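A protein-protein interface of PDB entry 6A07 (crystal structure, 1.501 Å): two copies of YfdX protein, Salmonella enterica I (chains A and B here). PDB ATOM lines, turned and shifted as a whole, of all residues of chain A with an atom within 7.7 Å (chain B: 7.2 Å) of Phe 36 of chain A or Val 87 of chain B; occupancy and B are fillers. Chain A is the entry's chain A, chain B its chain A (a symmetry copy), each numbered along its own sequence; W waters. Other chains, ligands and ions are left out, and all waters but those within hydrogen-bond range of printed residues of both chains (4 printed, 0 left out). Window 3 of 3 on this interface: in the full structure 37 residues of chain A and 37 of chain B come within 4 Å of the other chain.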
ATOM      1  N   MET A  30       7.403  13.437  11.799  1.00  0.00           N
ATOM      2  CA  MET A  30       6.384  12.398  11.895  1.00  0.00           C
ATOM      3  C   MET A  30       5.579  12.576  13.173  1.00  0.00           C
ATOM      4  O   MET A  30       4.357  12.398  13.174  1.00  0.00           O
ATOM      5  CB  MET A  30       7.023  11.006  11.841  1.00  0.00           C
ATOM      6  CG  MET A  30       7.744  10.678  10.525  1.00  0.00           C
ATOM      7  SD  MET A  30       8.191   8.927  10.425  1.00  0.00           S
ATOM      8  CE  MET A  30       6.669   8.293  11.152  1.00  0.00           C
ATOM      9  N   SER A  31       6.247  12.976  14.256  1.00  0.00           N
ATOM     10  CA  SER A  31       5.551  13.231  15.514  1.00  0.00           C
ATOM     11  C   SER A  31       4.503  14.321  15.334  1.00  0.00           C
ATOM     12  O   SER A  31       3.348  14.179  15.766  1.00  0.00           O
ATOM     13  CB  SER A  31       6.573  13.617  16.590  1.00  0.00           C
ATOM     14  OG  SER A  31       5.963  13.946  17.827  1.00  0.00           O
ATOM     15  N   ARG A  32       4.879  15.414  14.666  1.00  0.00           N
ATOM     16  CA  ARG A  32       3.924  16.499  14.484  1.00  0.00           C
ATOM     17  C   ARG A  32       2.720  16.025  13.688  1.00  0.00           C
ATOM     18  O   ARG A  32       1.574  16.319  14.044  1.00  0.00           O
ATOM     19  CB  ARG A  32       4.582  17.693  13.791  1.00  0.00           C
ATOM     20  CG  ARG A  32       3.613  18.834  13.622  1.00  0.00           C
ATOM     21  CD  ARG A  32       4.351  20.112  13.277  1.00  0.00           C
ATOM     22  NE  ARG A  32       3.439  21.203  12.977  1.00  0.00           N
ATOM     23  CZ  ARG A  32       2.985  21.469  11.753  1.00  0.00           C
ATOM     24  NH1 ARG A  32       3.357  20.715  10.730  1.00  0.00           N
ATOM     25  NH2 ARG A  32       2.158  22.485  11.556  1.00  0.00           N
ATOM     26  N   PHE A  33       2.960  15.269  12.615  1.00  0.00           N
ATOM     27  CA  PHE A  33       1.840  14.773  11.826  1.00  0.00           C
ATOM     28  C   PHE A  33       0.896  13.931  12.669  1.00  0.00           C
ATOM     29  O   PHE A  33      -0.334  14.058  12.557  1.00  0.00           O
ATOM     30  CB  PHE A  33       2.337  13.957  10.635  1.00  0.00           C
ATOM     31  CG  PHE A  33       1.215  13.340   9.846  1.00  0.00           C
ATOM     32  CD1 PHE A  33       0.476  14.113   8.961  1.00  0.00           C
ATOM     33  CD2 PHE A  33       0.868  12.010  10.026  1.00  0.00           C
ATOM     34  CE1 PHE A  33      -0.589  13.558   8.250  1.00  0.00           C
ATOM     35  CE2 PHE A  33      -0.198  11.455   9.310  1.00  0.00           C
ATOM     36  CZ  PHE A  33      -0.920  12.239   8.427  1.00  0.00           C
ATOM     37  N   GLU A  34       1.450  13.065  13.521  1.00  0.00           N
ATOM     38  CA  GLU A  34       0.605  12.150  14.281  1.00  0.00           C
ATOM     39  C   GLU A  34      -0.266  12.878  15.305  1.00  0.00           C
ATOM     40  O   GLU A  34      -1.324  12.360  15.665  1.00  0.00           O
ATOM     41  CB  GLU A  34       1.466  11.069  14.944  1.00  0.00           C
ATOM     42  CG  GLU A  34       2.176  10.145  13.955  1.00  0.00           C
ATOM     43  CD  GLU A  34       1.248   9.358  13.045  1.00  0.00           C
ATOM     44  OE1 GLU A  34       0.012   9.400  13.220  1.00  0.00           O
ATOM     45  OE2 GLU A  34       1.770   8.667  12.142  1.00  0.00           O
ATOM     46  N   LEU A  35       0.129  14.073  15.758  1.00  0.00           N
ATOM     47  CA  LEU A  35      -0.757  14.872  16.608  1.00  0.00           C
ATOM     48  C   LEU A  35      -2.063  15.179  15.889  1.00  0.00           C
ATOM     49  O   LEU A  35      -3.154  14.985  16.439  1.00  0.00           O
ATOM     50  CB  LEU A  35      -0.076  16.177  17.032  1.00  0.00           C
ATOM     51  CG  LEU A  35       1.188  16.053  17.872  1.00  0.00           C
ATOM     52  CD1 LEU A  35       1.859  17.398  18.042  1.00  0.00           C
ATOM     53  CD2 LEU A  35       0.862  15.450  19.235  1.00  0.00           C
ATOM     54  N   PHE A  36      -1.972  15.653  14.645  1.00  0.00           N
ATOM     55  CA  PHE A  36      -3.165  15.957  13.867  1.00  0.00           C
ATOM     56  C   PHE A  36      -3.885  14.705  13.397  1.00  0.00           C
ATOM     57  O   PHE A  36      -5.082  14.767  13.110  1.00  0.00           O
ATOM     58  CB  PHE A  36      -2.769  16.826  12.664  1.00  0.00           C
ATOM     59  CG  PHE A  36      -2.260  18.181  13.050  1.00  0.00           C
ATOM     60  CD1 PHE A  36      -3.143  19.236  13.200  1.00  0.00           C
ATOM     61  CD2 PHE A  36      -0.912  18.404  13.289  1.00  0.00           C
ATOM     62  CE1 PHE A  36      -2.696  20.489  13.573  1.00  0.00           C
ATOM     63  CE2 PHE A  36      -0.451  19.661  13.648  1.00  0.00           C
ATOM     64  CZ  PHE A  36      -1.347  20.705  13.802  1.00  0.00           C
ATOM     65  N   ASN A  37      -3.182  13.581  13.301  1.00  0.00           N
ATOM     66  CA  ASN A  37      -3.737  12.308  12.854  1.00  0.00           C
ATOM     67  C   ASN A  37      -4.461  11.564  13.971  1.00  0.00           C
ATOM     68  O   ASN A  37      -4.815  10.392  13.793  1.00  0.00           O
ATOM     69  CB  ASN A  37      -2.602  11.452  12.287  1.00  0.00           C
ATOM     70  CG  ASN A  37      -3.078  10.378  11.341  1.00  0.00           C
ATOM     71  OD1 ASN A  37      -4.087  10.531  10.645  1.00  0.00           O
ATOM     72  ND2 ASN A  37      -2.329   9.278  11.288  1.00  0.00           N
ATOM     73  N   GLY A  38      -4.652  12.211  15.114  1.00  0.00           N
ATOM     74  CA  GLY A  38      -5.338  11.579  16.224  1.00  0.00           C
ATOM     75  C   GLY A  38      -4.570  10.457  16.879  1.00  0.00           C
ATOM     76  O   GLY A  38      -5.180   9.587  17.506  1.00  0.00           O
ATOM     77  N   ARG A  39      -3.248  10.452  16.760  1.00  0.00           N
ATOM     78  CA  ARG A  39      -2.394   9.416  17.340  1.00  0.00           C
ATOM     79  C   ARG A  39      -1.367  10.086  18.250  1.00  0.00           C
ATOM     80  O   ARG A  39      -0.158  10.026  17.988  1.00  0.00           O
ATOM     81  CB  ARG A  39      -1.721   8.578  16.238  1.00  0.00           C
ATOM     82  CG  ARG A  39      -2.682   7.684  15.466  1.00  0.00           C
ATOM     83  CD  ARG A  39      -1.998   7.063  14.260  1.00  0.00           C
ATOM     84  NE  ARG A  39      -2.681   5.864  13.769  1.00  0.00           N
ATOM     85  CZ  ARG A  39      -3.703   5.869  12.917  1.00  0.00           C
ATOM     86  NH1 ARG A  39      -4.193   7.017  12.463  1.00  0.00           N
ATOM     87  NH2 ARG A  39      -4.248   4.721  12.529  1.00  0.00           N
ATOM     88  N   THR A  40      -1.848  10.706  19.337  1.00  0.00           N
ATOM     89  CA  THR A  40      -0.942  11.456  20.207  1.00  0.00           C
ATOM     90  C   THR A  40       0.048  10.547  20.922  1.00  0.00           C
ATOM     91  O   THR A  40       1.171  10.969  21.210  1.00  0.00           O
ATOM     92  CB  THR A  40      -1.711  12.292  21.237  1.00  0.00           C
ATOM     93  OG1 THR A  40      -2.521  11.434  22.056  1.00  0.00           O
ATOM     94  CG2 THR A  40      -2.569  13.337  20.553  1.00  0.00           C
ATOM     95  N   ALA A  43       2.720  10.050  18.593  1.00  0.00           N
ATOM     96  CA  ALA A  43       3.514  11.275  18.520  1.00  0.00           C
ATOM     97  C   ALA A  43       4.515  11.347  19.662  1.00  0.00           C
ATOM     98  O   ALA A  43       5.663  11.749  19.469  1.00  0.00           O
ATOM     99  CB  ALA A  43       2.608  12.502  18.532  1.00  0.00           C
ATOM    100  N   TYR A 155      -1.404  19.527  23.071  1.00  0.00           N
ATOM    101  CA  TYR A 155      -0.871  18.909  21.858  1.00  0.00           C
ATOM    102  C   TYR A 155      -0.627  19.935  20.755  1.00  0.00           C
ATOM    103  O   TYR A 155       0.402  19.870  20.066  1.00  0.00           O
ATOM    104  CB  TYR A 155      -1.811  17.810  21.380  1.00  0.00           C
ATOM    105  CG  TYR A 155      -1.981  16.711  22.407  1.00  0.00           C
ATOM    106  CD1 TYR A 155      -0.920  15.885  22.735  1.00  0.00           C
ATOM    107  CD2 TYR A 155      -3.198  16.507  23.043  1.00  0.00           C
ATOM    108  CE1 TYR A 155      -1.063  14.876  23.675  1.00  0.00           C
ATOM    109  CE2 TYR A 155      -3.346  15.503  23.983  1.00  0.00           C
ATOM    110  CZ  TYR A 155      -2.272  14.700  24.292  1.00  0.00           C
ATOM    111  OH  TYR A 155      -2.395  13.686  25.228  1.00  0.00           O
ATOM    112  N   TYR A 156      -1.549  20.883  20.568  1.00  0.00           N
ATOM    113  CA  TYR A 156      -1.334  21.890  19.528  1.00  0.00           C
ATOM    114  C   TYR A 156      -0.076  22.700  19.815  1.00  0.00           C
ATOM    115  O   TYR A 156       0.730  22.971  18.908  1.00  0.00           O
ATOM    116  CB  TYR A 156      -2.551  22.814  19.420  1.00  0.00           C
ATOM    117  CG  TYR A 156      -2.488  23.691  18.198  1.00  0.00           C
ATOM    118  CD1 TYR A 156      -2.858  23.198  16.955  1.00  0.00           C
ATOM    119  CD2 TYR A 156      -2.046  25.006  18.287  1.00  0.00           C
ATOM    120  CE1 TYR A 156      -2.792  24.000  15.817  1.00  0.00           C
ATOM    121  CE2 TYR A 156      -1.972  25.809  17.161  1.00  0.00           C
ATOM    122  CZ  TYR A 156      -2.346  25.295  15.934  1.00  0.00           C
ATOM    123  OH  TYR A 156      -2.279  26.093  14.805  1.00  0.00           O
ATOM    124  N   ALA A 158       2.525  21.695  21.516  1.00  0.00           N
ATOM    125  CA  ALA A 158       3.638  20.816  21.185  1.00  0.00           C
ATOM    126  C   ALA A 158       3.929  20.832  19.688  1.00  0.00           C
ATOM    127  O   ALA A 158       5.095  20.896  19.278  1.00  0.00           O
ATOM    128  CB  ALA A 158       3.335  19.394  21.657  1.00  0.00           C
ATOM    129  N   GLY A 159       2.879  20.767  18.868  1.00  0.00           N
ATOM    130  CA  GLY A 159       3.066  20.793  17.422  1.00  0.00           C
ATOM    131  C   GLY A 159       3.740  22.057  16.947  1.00  0.00           C
ATOM    132  O   GLY A 159       4.538  22.025  16.004  1.00  0.00           O
ATOM    133  N   LEU A 160       3.428  23.196  17.578  1.00  0.00           N
ATOM    134  CA  LEU A 160       4.093  24.446  17.224  1.00  0.00           C
ATOM    135  C   LEU A 160       5.593  24.368  17.476  1.00  0.00           C
ATOM    136  O   LEU A 160       6.393  24.855  16.664  1.00  0.00           O
ATOM    137  CB  LEU A 160       3.488  25.616  18.002  1.00  0.00           C
ATOM    138  CG  LEU A 160       2.037  25.968  17.727  1.00  0.00           C
ATOM    139  CD1 LEU A 160       1.595  27.037  18.718  1.00  0.00           C
ATOM    140  CD2 LEU A 160       1.862  26.469  16.300  1.00  0.00           C
ATOM    141  N   LYS A 163       7.226  22.171  14.872  1.00  0.00           N
ATOM    142  CA  LYS A 163       7.370  22.914  13.622  1.00  0.00           C
ATOM    143  C   LYS A 163       8.524  23.902  13.717  1.00  0.00           C
ATOM    144  O   LYS A 163       9.317  24.040  12.771  1.00  0.00           O
ATOM    145  CB  LYS A 163       6.059  23.640  13.294  1.00  0.00           C
ATOM    146  CG  LYS A 163       6.064  24.373  11.946  1.00  0.00           C
ATOM    147  CD  LYS A 163       6.278  23.413  10.786  1.00  0.00           C
ATOM    148  CE  LYS A 163       6.208  24.140   9.440  1.00  0.00           C
ATOM    149  NZ  LYS A 163       6.321  23.179   8.302  1.00  0.00           N
ATOM    150  N   LEU B  12      -4.413  11.222   6.774  1.00  0.00           N
ATOM    151  CA  LEU B  12      -5.576  11.576   7.584  1.00  0.00           C
ATOM    152  C   LEU B  12      -6.807  10.776   7.177  1.00  0.00           C
ATOM    153  O   LEU B  12      -7.657  10.476   8.025  1.00  0.00           O
ATOM    154  CB  LEU B  12      -5.859  13.077   7.485  1.00  0.00           C
ATOM    155  CG  LEU B  12      -4.756  14.007   8.000  1.00  0.00           C
ATOM    156  CD1 LEU B  12      -5.101  15.477   7.745  1.00  0.00           C
ATOM    157  CD2 LEU B  12      -4.477  13.758   9.477  1.00  0.00           C
ATOM    158  N   SER B  84       2.570  15.410   5.678  1.00  0.00           N
ATOM    159  CA  SER B  84       2.826  16.453   6.662  1.00  0.00           C
ATOM    160  C   SER B  84       1.633  17.395   6.711  1.00  0.00           C
ATOM    161  O   SER B  84       0.718  17.315   5.890  1.00  0.00           O
ATOM    162  CB  SER B  84       4.099  17.243   6.345  1.00  0.00           C
ATOM    163  OG  SER B  84       3.911  18.045   5.186  1.00  0.00           O
ATOM    164  N   ILE B  85       1.661  18.312   7.679  1.00  0.00           N
ATOM    165  CA  ILE B  85       0.563  19.238   7.926  1.00  0.00           C
ATOM    166  C   ILE B  85       1.048  20.665   7.725  1.00  0.00           C
ATOM    167  O   ILE B  85       2.148  21.020   8.161  1.00  0.00           O
ATOM    168  CB  ILE B  85       0.003  19.077   9.358  1.00  0.00           C
ATOM    169  CG1 ILE B  85      -0.555  17.665   9.554  1.00  0.00           C
ATOM    170  CG2 ILE B  85      -1.044  20.153   9.680  1.00  0.00           C
ATOM    171  CD1 ILE B  85      -1.742  17.378   8.702  1.00  0.00           C
ATOM    172  N   THR B  86       0.230  21.473   7.057  1.00  0.00           N
ATOM    173  CA  THR B  86       0.338  22.930   7.107  1.00  0.00           C
ATOM    174  C   THR B  86      -0.882  23.518   7.801  1.00  0.00           C
ATOM    175  O   THR B  86      -2.021  23.221   7.424  1.00  0.00           O
ATOM    176  CB  THR B  86       0.456  23.519   5.705  1.00  0.00           C
ATOM    177  OG1 THR B  86       1.654  23.037   5.111  1.00  0.00           O
ATOM    178  CG2 THR B  86       0.491  25.061   5.755  1.00  0.00           C
ATOM    179  N   VAL B  87      -0.658  24.366   8.805  1.00  0.00           N
ATOM    180  CA  VAL B  87      -1.761  25.086   9.430  1.00  0.00           C
ATOM    181  C   VAL B  87      -1.738  26.537   8.965  1.00  0.00           C
ATOM    182  O   VAL B  87      -0.682  27.104   8.656  1.00  0.00           O
ATOM    183  CB  VAL B  87      -1.738  25.010  10.973  1.00  0.00           C
ATOM    184  CG1 VAL B  87      -1.943  23.575  11.424  1.00  0.00           C
ATOM    185  CG2 VAL B  87      -0.436  25.597  11.526  1.00  0.00           C
ATOM    186  N   ALA B  88      -2.929  27.123   8.879  1.00  0.00           N
ATOM    187  CA  ALA B  88      -3.091  28.551   8.617  1.00  0.00           C
ATOM    188  C   ALA B  88      -3.934  29.152   9.730  1.00  0.00           C
ATOM    189  O   ALA B  88      -5.117  28.821   9.866  1.00  0.00           O
ATOM    190  CB  ALA B  88      -3.747  28.792   7.257  1.00  0.00           C
ATOM    191  N   GLU B  89      -3.338  30.052  10.508  1.00  0.00           N
ATOM    192  CA  GLU B  89      -3.962  30.591  11.713  1.00  0.00           C
ATOM    193  C   GLU B  89      -4.502  31.997  11.455  1.00  0.00           C
ATOM    194  O   GLU B  89      -3.730  32.929  11.213  1.00  0.00           O
ATOM    195  CB  GLU B  89      -2.964  30.609  12.866  1.00  0.00           C
ATOM    196  CG  GLU B  89      -2.456  29.234  13.261  1.00  0.00           C
ATOM    197  CD  GLU B  89      -1.826  29.237  14.637  1.00  0.00           C
ATOM    198  OE1 GLU B  89      -2.155  30.137  15.439  1.00  0.00           O
ATOM    199  OE2 GLU B  89      -1.005  28.342  14.920  1.00  0.00           O
ATOM    200  N   MET B 108      -7.828  15.786  19.844  1.00  0.00           N
ATOM    201  CA  MET B 108      -6.635  15.026  19.485  1.00  0.00           C
ATOM    202  C   MET B 108      -6.369  13.915  20.494  1.00  0.00           C
ATOM    203  O   MET B 108      -6.035  12.789  20.110  1.00  0.00           O
ATOM    204  CB  MET B 108      -5.430  15.956  19.371  1.00  0.00           C
ATOM    205  CG  MET B 108      -5.382  16.680  18.045  1.00  0.00           C
ATOM    206  SD  MET B 108      -3.934  17.740  17.863  1.00  0.00           S
ATOM    207  CE  MET B 108      -4.505  19.192  18.742  1.00  0.00           C
ATOM    208  N   ASP B 112      -9.963  11.729  17.554  1.00  0.00           N
ATOM    209  CA  ASP B 112     -11.102  12.146  16.739  1.00  0.00           C
ATOM    210  C   ASP B 112     -10.599  13.137  15.696  1.00  0.00           C
ATOM    211  O   ASP B 112     -10.589  14.346  15.925  1.00  0.00           O
ATOM    212  CB  ASP B 112     -12.171  12.757  17.638  1.00  0.00           C
ATOM    213  CG  ASP B 112     -13.414  13.172  16.886  1.00  0.00           C
ATOM    214  OD1 ASP B 112     -13.490  12.966  15.654  1.00  0.00           O
ATOM    215  OD2 ASP B 112     -14.327  13.702  17.553  1.00  0.00           O
ATOM    216  N   LYS B 113     -10.195  12.615  14.534  1.00  0.00           N
ATOM    217  CA  LYS B 113      -9.594  13.462  13.506  1.00  0.00           C
ATOM    218  C   LYS B 113     -10.575  14.517  13.020  1.00  0.00           C
ATOM    219  O   LYS B 113     -10.239  15.701  12.927  1.00  0.00           O
ATOM    220  CB  LYS B 113      -9.122  12.620  12.320  1.00  0.00           C
ATOM    221  CG  LYS B 113      -8.024  11.634  12.607  1.00  0.00           C
ATOM    222  CD  LYS B 113      -7.578  10.999  11.293  1.00  0.00           C
ATOM    223  CE  LYS B 113      -7.126   9.559  11.472  1.00  0.00           C
ATOM    224  NZ  LYS B 113      -6.362   9.041  10.283  1.00  0.00           N
ATOM    225  N   LYS B 114     -11.794  14.092  12.682  1.00  0.00           N
ATOM    226  CA  LYS B 114     -12.820  15.026  12.240  1.00  0.00           C
ATOM    227  C   LYS B 114     -13.084  16.089  13.301  1.00  0.00           C
ATOM    228  O   LYS B 114     -13.159  17.284  12.995  1.00  0.00           O
ATOM    229  CB  LYS B 114     -14.096  14.255  11.899  1.00  0.00           C
ATOM    230  CG  LYS B 114     -15.292  15.121  11.566  1.00  0.00           C
ATOM    231  CD  LYS B 114     -15.097  15.876  10.268  1.00  0.00           C
ATOM    232  CE  LYS B 114     -16.379  16.583   9.858  1.00  0.00           C
ATOM    233  NZ  LYS B 114     -17.544  15.651   9.834  1.00  0.00           N
ATOM    234  N   THR B 116     -11.058  17.123  15.584  1.00  0.00           N
ATOM    235  CA  THR B 116      -9.897  18.004  15.672  1.00  0.00           C
ATOM    236  C   THR B 116      -9.960  19.097  14.612  1.00  0.00           C
ATOM    237  O   THR B 116      -9.757  20.280  14.906  1.00  0.00           O
ATOM    238  CB  THR B 116      -8.609  17.188  15.524  1.00  0.00           C
ATOM    239  OG1 THR B 116      -8.486  16.288  16.630  1.00  0.00           O
ATOM    240  CG2 THR B 116      -7.392  18.101  15.494  1.00  0.00           C
ATOM    241  N   ILE B 117     -10.245  18.712  13.365  1.00  0.00           N
ATOM    242  CA  ILE B 117     -10.339  19.693  12.287  1.00  0.00           C
ATOM    243  C   ILE B 117     -11.426  20.714  12.592  1.00  0.00           C
ATOM    244  O   ILE B 117     -11.239  21.921  12.397  1.00  0.00           O
ATOM    245  CB  ILE B 117     -10.574  18.984  10.941  1.00  0.00           C
ATOM    246  CG1 ILE B 117      -9.470  17.956  10.685  1.00  0.00           C
ATOM    247  CG2 ILE B 117     -10.648  19.991   9.800  1.00  0.00           C
ATOM    248  CD1 ILE B 117      -8.059  18.506  10.821  1.00  0.00           C
ATOM    249  N   LEU B 120     -10.337  23.022  15.463  1.00  0.00           N
ATOM    250  CA  LEU B 120      -9.317  23.944  14.979  1.00  0.00           C
ATOM    251  C   LEU B 120      -9.935  25.058  14.145  1.00  0.00           C
ATOM    252  O   LEU B 120      -9.504  26.214  14.231  1.00  0.00           O
ATOM    253  CB  LEU B 120      -8.253  23.187  14.183  1.00  0.00           C
ATOM    254  CG  LEU B 120      -7.283  22.405  15.073  1.00  0.00           C
ATOM    255  CD1 LEU B 120      -6.318  21.578  14.226  1.00  0.00           C
ATOM    256  CD2 LEU B 120      -6.511  23.338  16.001  1.00  0.00           C
ATOM    257  N   VAL B 125      -8.104  28.118  12.664  1.00  0.00           N
ATOM    258  CA  VAL B 125      -6.988  27.355  12.111  1.00  0.00           C
ATOM    259  C   VAL B 125      -7.522  26.431  11.024  1.00  0.00           C
ATOM    260  O   VAL B 125      -8.342  25.549  11.302  1.00  0.00           O
ATOM    261  CB  VAL B 125      -6.276  26.547  13.207  1.00  0.00           C
ATOM    262  CG1 VAL B 125      -5.120  25.746  12.624  1.00  0.00           C
ATOM    263  CG2 VAL B 125      -5.796  27.474  14.323  1.00  0.00           C
ATOM    264  N   SER B 126      -7.051  26.618   9.792  1.00  0.00           N
ATOM    265  CA  SER B 126      -7.318  25.657   8.728  1.00  0.00           C
ATOM    266  C   SER B 126      -6.147  24.681   8.613  1.00  0.00           C
ATOM    267  O   SER B 126      -5.002  25.011   8.936  1.00  0.00           O
ATOM    268  CB  SER B 126      -7.557  26.361   7.391  1.00  0.00           C
ATOM    269  OG  SER B 126      -6.376  26.987   6.938  1.00  0.00           O
ATOM    270  N   VAL B 127      -6.446  23.472   8.147  1.00  0.00           N
ATOM    271  CA  VAL B 127      -5.462  22.389   8.072  1.00  0.00           C
ATOM    272  C   VAL B 127      -5.362  21.921   6.627  1.00  0.00           C
ATOM    273  O   VAL B 127      -6.377  21.634   5.986  1.00  0.00           O
ATOM    274  CB  VAL B 127      -5.826  21.209   8.994  1.00  0.00           C
ATOM    275  CG1 VAL B 127      -4.841  20.064   8.805  1.00  0.00           C
ATOM    276  CG2 VAL B 127      -5.840  21.650  10.446  1.00  0.00           C
ATOM    277  N   ILE B 128      -4.133  21.842   6.123  1.00  0.00           N
ATOM    278  CA  ILE B 128      -3.829  21.283   4.811  1.00  0.00           C
ATOM    279  C   ILE B 128      -2.901  20.097   5.008  1.00  0.00           C
ATOM    280  O   ILE B 128      -1.950  20.170   5.793  1.00  0.00           O
ATOM    281  CB  ILE B 128      -3.177  22.344   3.895  1.00  0.00           C
ATOM    282  CG1 ILE B 128      -4.183  23.424   3.504  1.00  0.00           C
ATOM    283  CG2 ILE B 128      -2.535  21.700   2.663  1.00  0.00           C
ATOM    284  CD1 ILE B 128      -5.183  22.967   2.495  1.00  0.00           C
ATOM    285  N   ASN B 130      -0.134  17.700   3.277  1.00  0.00           N
ATOM    286  CA  ASN B 130       0.825  17.683   2.170  1.00  0.00           C
ATOM    287  C   ASN B 130       1.297  16.255   1.967  1.00  0.00           C
ATOM    288  O   ASN B 130       2.021  15.716   2.807  1.00  0.00           O
ATOM    289  CB  ASN B 130       2.021  18.583   2.450  1.00  0.00           C
ATOM    290  CG  ASN B 130       1.619  19.953   2.900  1.00  0.00           C
ATOM    291  OD1 ASN B 130       1.032  20.715   2.150  1.00  0.00           O
ATOM    292  ND2 ASN B 130       1.951  20.282   4.153  1.00  0.00           N
ATOM    293  N   LEU B 178     -12.591  14.875   5.693  1.00  0.00           N
ATOM    294  CA  LEU B 178     -12.665  13.573   6.352  1.00  0.00           C
ATOM    295  C   LEU B 178     -14.074  12.990   6.312  1.00  0.00           C
ATOM    296  O   LEU B 178     -14.319  11.987   5.634  1.00  0.00           O
ATOM    297  CB  LEU B 178     -12.169  13.690   7.795  1.00  0.00           C
ATOM    298  CG  LEU B 178     -10.707  14.137   7.881  1.00  0.00           C
ATOM    299  CD1 LEU B 178     -10.162  13.968   9.271  1.00  0.00           C
ATOM    300  CD2 LEU B 178      -9.841  13.363   6.890  1.00  0.00           C
HETATM  301  O   HOH W   1       5.035  21.170   7.067  1.00  0.00           O
HETATM  302  O   HOH W   2       3.875  24.145   6.655  1.00  0.00           O
HETATM  303  O   HOH W   3      -4.683  10.403  20.283  1.00  0.00           O
HETATM  304  O   HOH W   4      -6.948  14.168  15.466  1.00  0.00           O
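Phe 36 of chain A touches just these residues of chain B: Leu 12, Ile 85, Val 87 and Leu 120. Printed residues of chain A within 4 Å of Leu 12 of chain B: Phe 33, Phe 36 and Asn 37. Printed residues of chain B within 4 Å of Arg 39 of chain A: Lys 113 (3.7 Å). Of the printed residues of chain B, Tyr 156 of chain A touches Val 87 (3.8 Å), Glu 89 (2.6 Å), Met 108 (3.9 Å), Leu 120 (3.8 Å) and Val 125 (3.6 Å). Printed residues of chain A within 4 Å of Lys 113 of chain B: Asn 37 and Arg 39. The nearest printed residue of chain B that does not touch Phe 36 of chain A is Met 108 of chain B (4.3 Å). The nearest printed residue of chain B that does not touch Leu 160 of chain A is Val 87 of chain B (5.4 Å).
The side-chain carboxylate (OE1) of Glu 34 of chain A sits at hydrogen-bond distance from the side-chain amide nitrogen (ND2) of Asn 37 of chain A (3.0 Å). The backbone carbonyl oxygen of Gly 159 of chain A sits at hydrogen-bond distance from the guanidinium group of Arg 32 of chain A (3.3 Å). N of Met 108 of chain B sits at hydrogen-bond distance from OG1 of Thr 116 of chain B (3.3 Å).
Hydrophobic or aromatic side chains of chain B that line the printed part of chain A: Leu 12, Ile 85, Val 87, Met 108, Leu 120 and Val 125. Along chain B the printed residues that touch a printed residue of chain A span positions 12 to 125. Hydrophobic or aromatic side chains of chain A within 4 Å of the printed part of chain B: Phe 33, Phe 36, Tyr 156 and Leu 160. Along chain A the printed residues that touch a printed residue of chain B span positions 32 to 160. Among the printed residues, no Asp or Glu carboxylate lies within 4 Å of a Lys or Arg side-chain nitrogen of the other chain.
Among the printed residues, merely in contact across the chains: Phe 33 of chain A with Leu 12 of chain B (3.996 Å), Phe 33 of chain A with Ile 85 of chain B (3.7 Å), Phe 36 of chain A with Leu 12 of chain B (3.8 Å), Phe 36 of chain A with Ile 85 of chain B (3.8 Å), Phe 36 of chain A with Val 87 of chain B (3.8 Å), Phe 36 of chain A with Leu 120 of chain B (3.8 Å), Asn 37 of chain A with Leu 12 of chain B (3.5 Å), Arg 39 of chain A with Lys 113 of chain B (3.7 Å), Thr 40 of chain A with Met 108 of chain B (3.5 Å), Tyr 156 of chain A with Val 87 of chain B (3.8 Å), Tyr 156 of chain A with Met 108 of chain B (3.9 Å), Tyr 156 of chain A with Leu 120 of chain B (3.8 Å), Tyr 156 of chain A with Val 125 of chain B (3.6 Å) and Leu 160 of chain A with Glu 89 of chain B (3.7 Å).
Water W3 lies within hydrogen-bond range of the backbone carbonyl oxygen of Met 108 of chain B (2.7 Å), the backbone carbonyl oxygen of Gly 38 of chain A (2.9 Å) and the side-chain hydroxyl of Thr 40 of chain A (3.0 Å). Water W2 lies within hydrogen-bond range of the side-chain hydroxyl of Thr 86 of chain B and the side-chain amino group of Lys 163 of chain A.
No position is printed for both chains. Of the 18 pairs that touch across the chains among the printed residues, none has its exchanged pair printed and touching as well.
NH1 of Arg 32 of chain A is in hydrogen-bond range of O of Ile 85 of chain B. The backbone carbonyl oxygen (O) of Leu 35 of chain A lies close to the side-chain sulfur (SD) of Met 108 of chain B (3.2 Å). OH of Tyr 156 of chain A sits at hydrogen-bond distance from OE2 of Glu 89 of chain B. OD1 of Asn 37 of chain A sits at hydrogen-bond distance from NZ of Lys 113 of chain B, at 2.7 Å.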
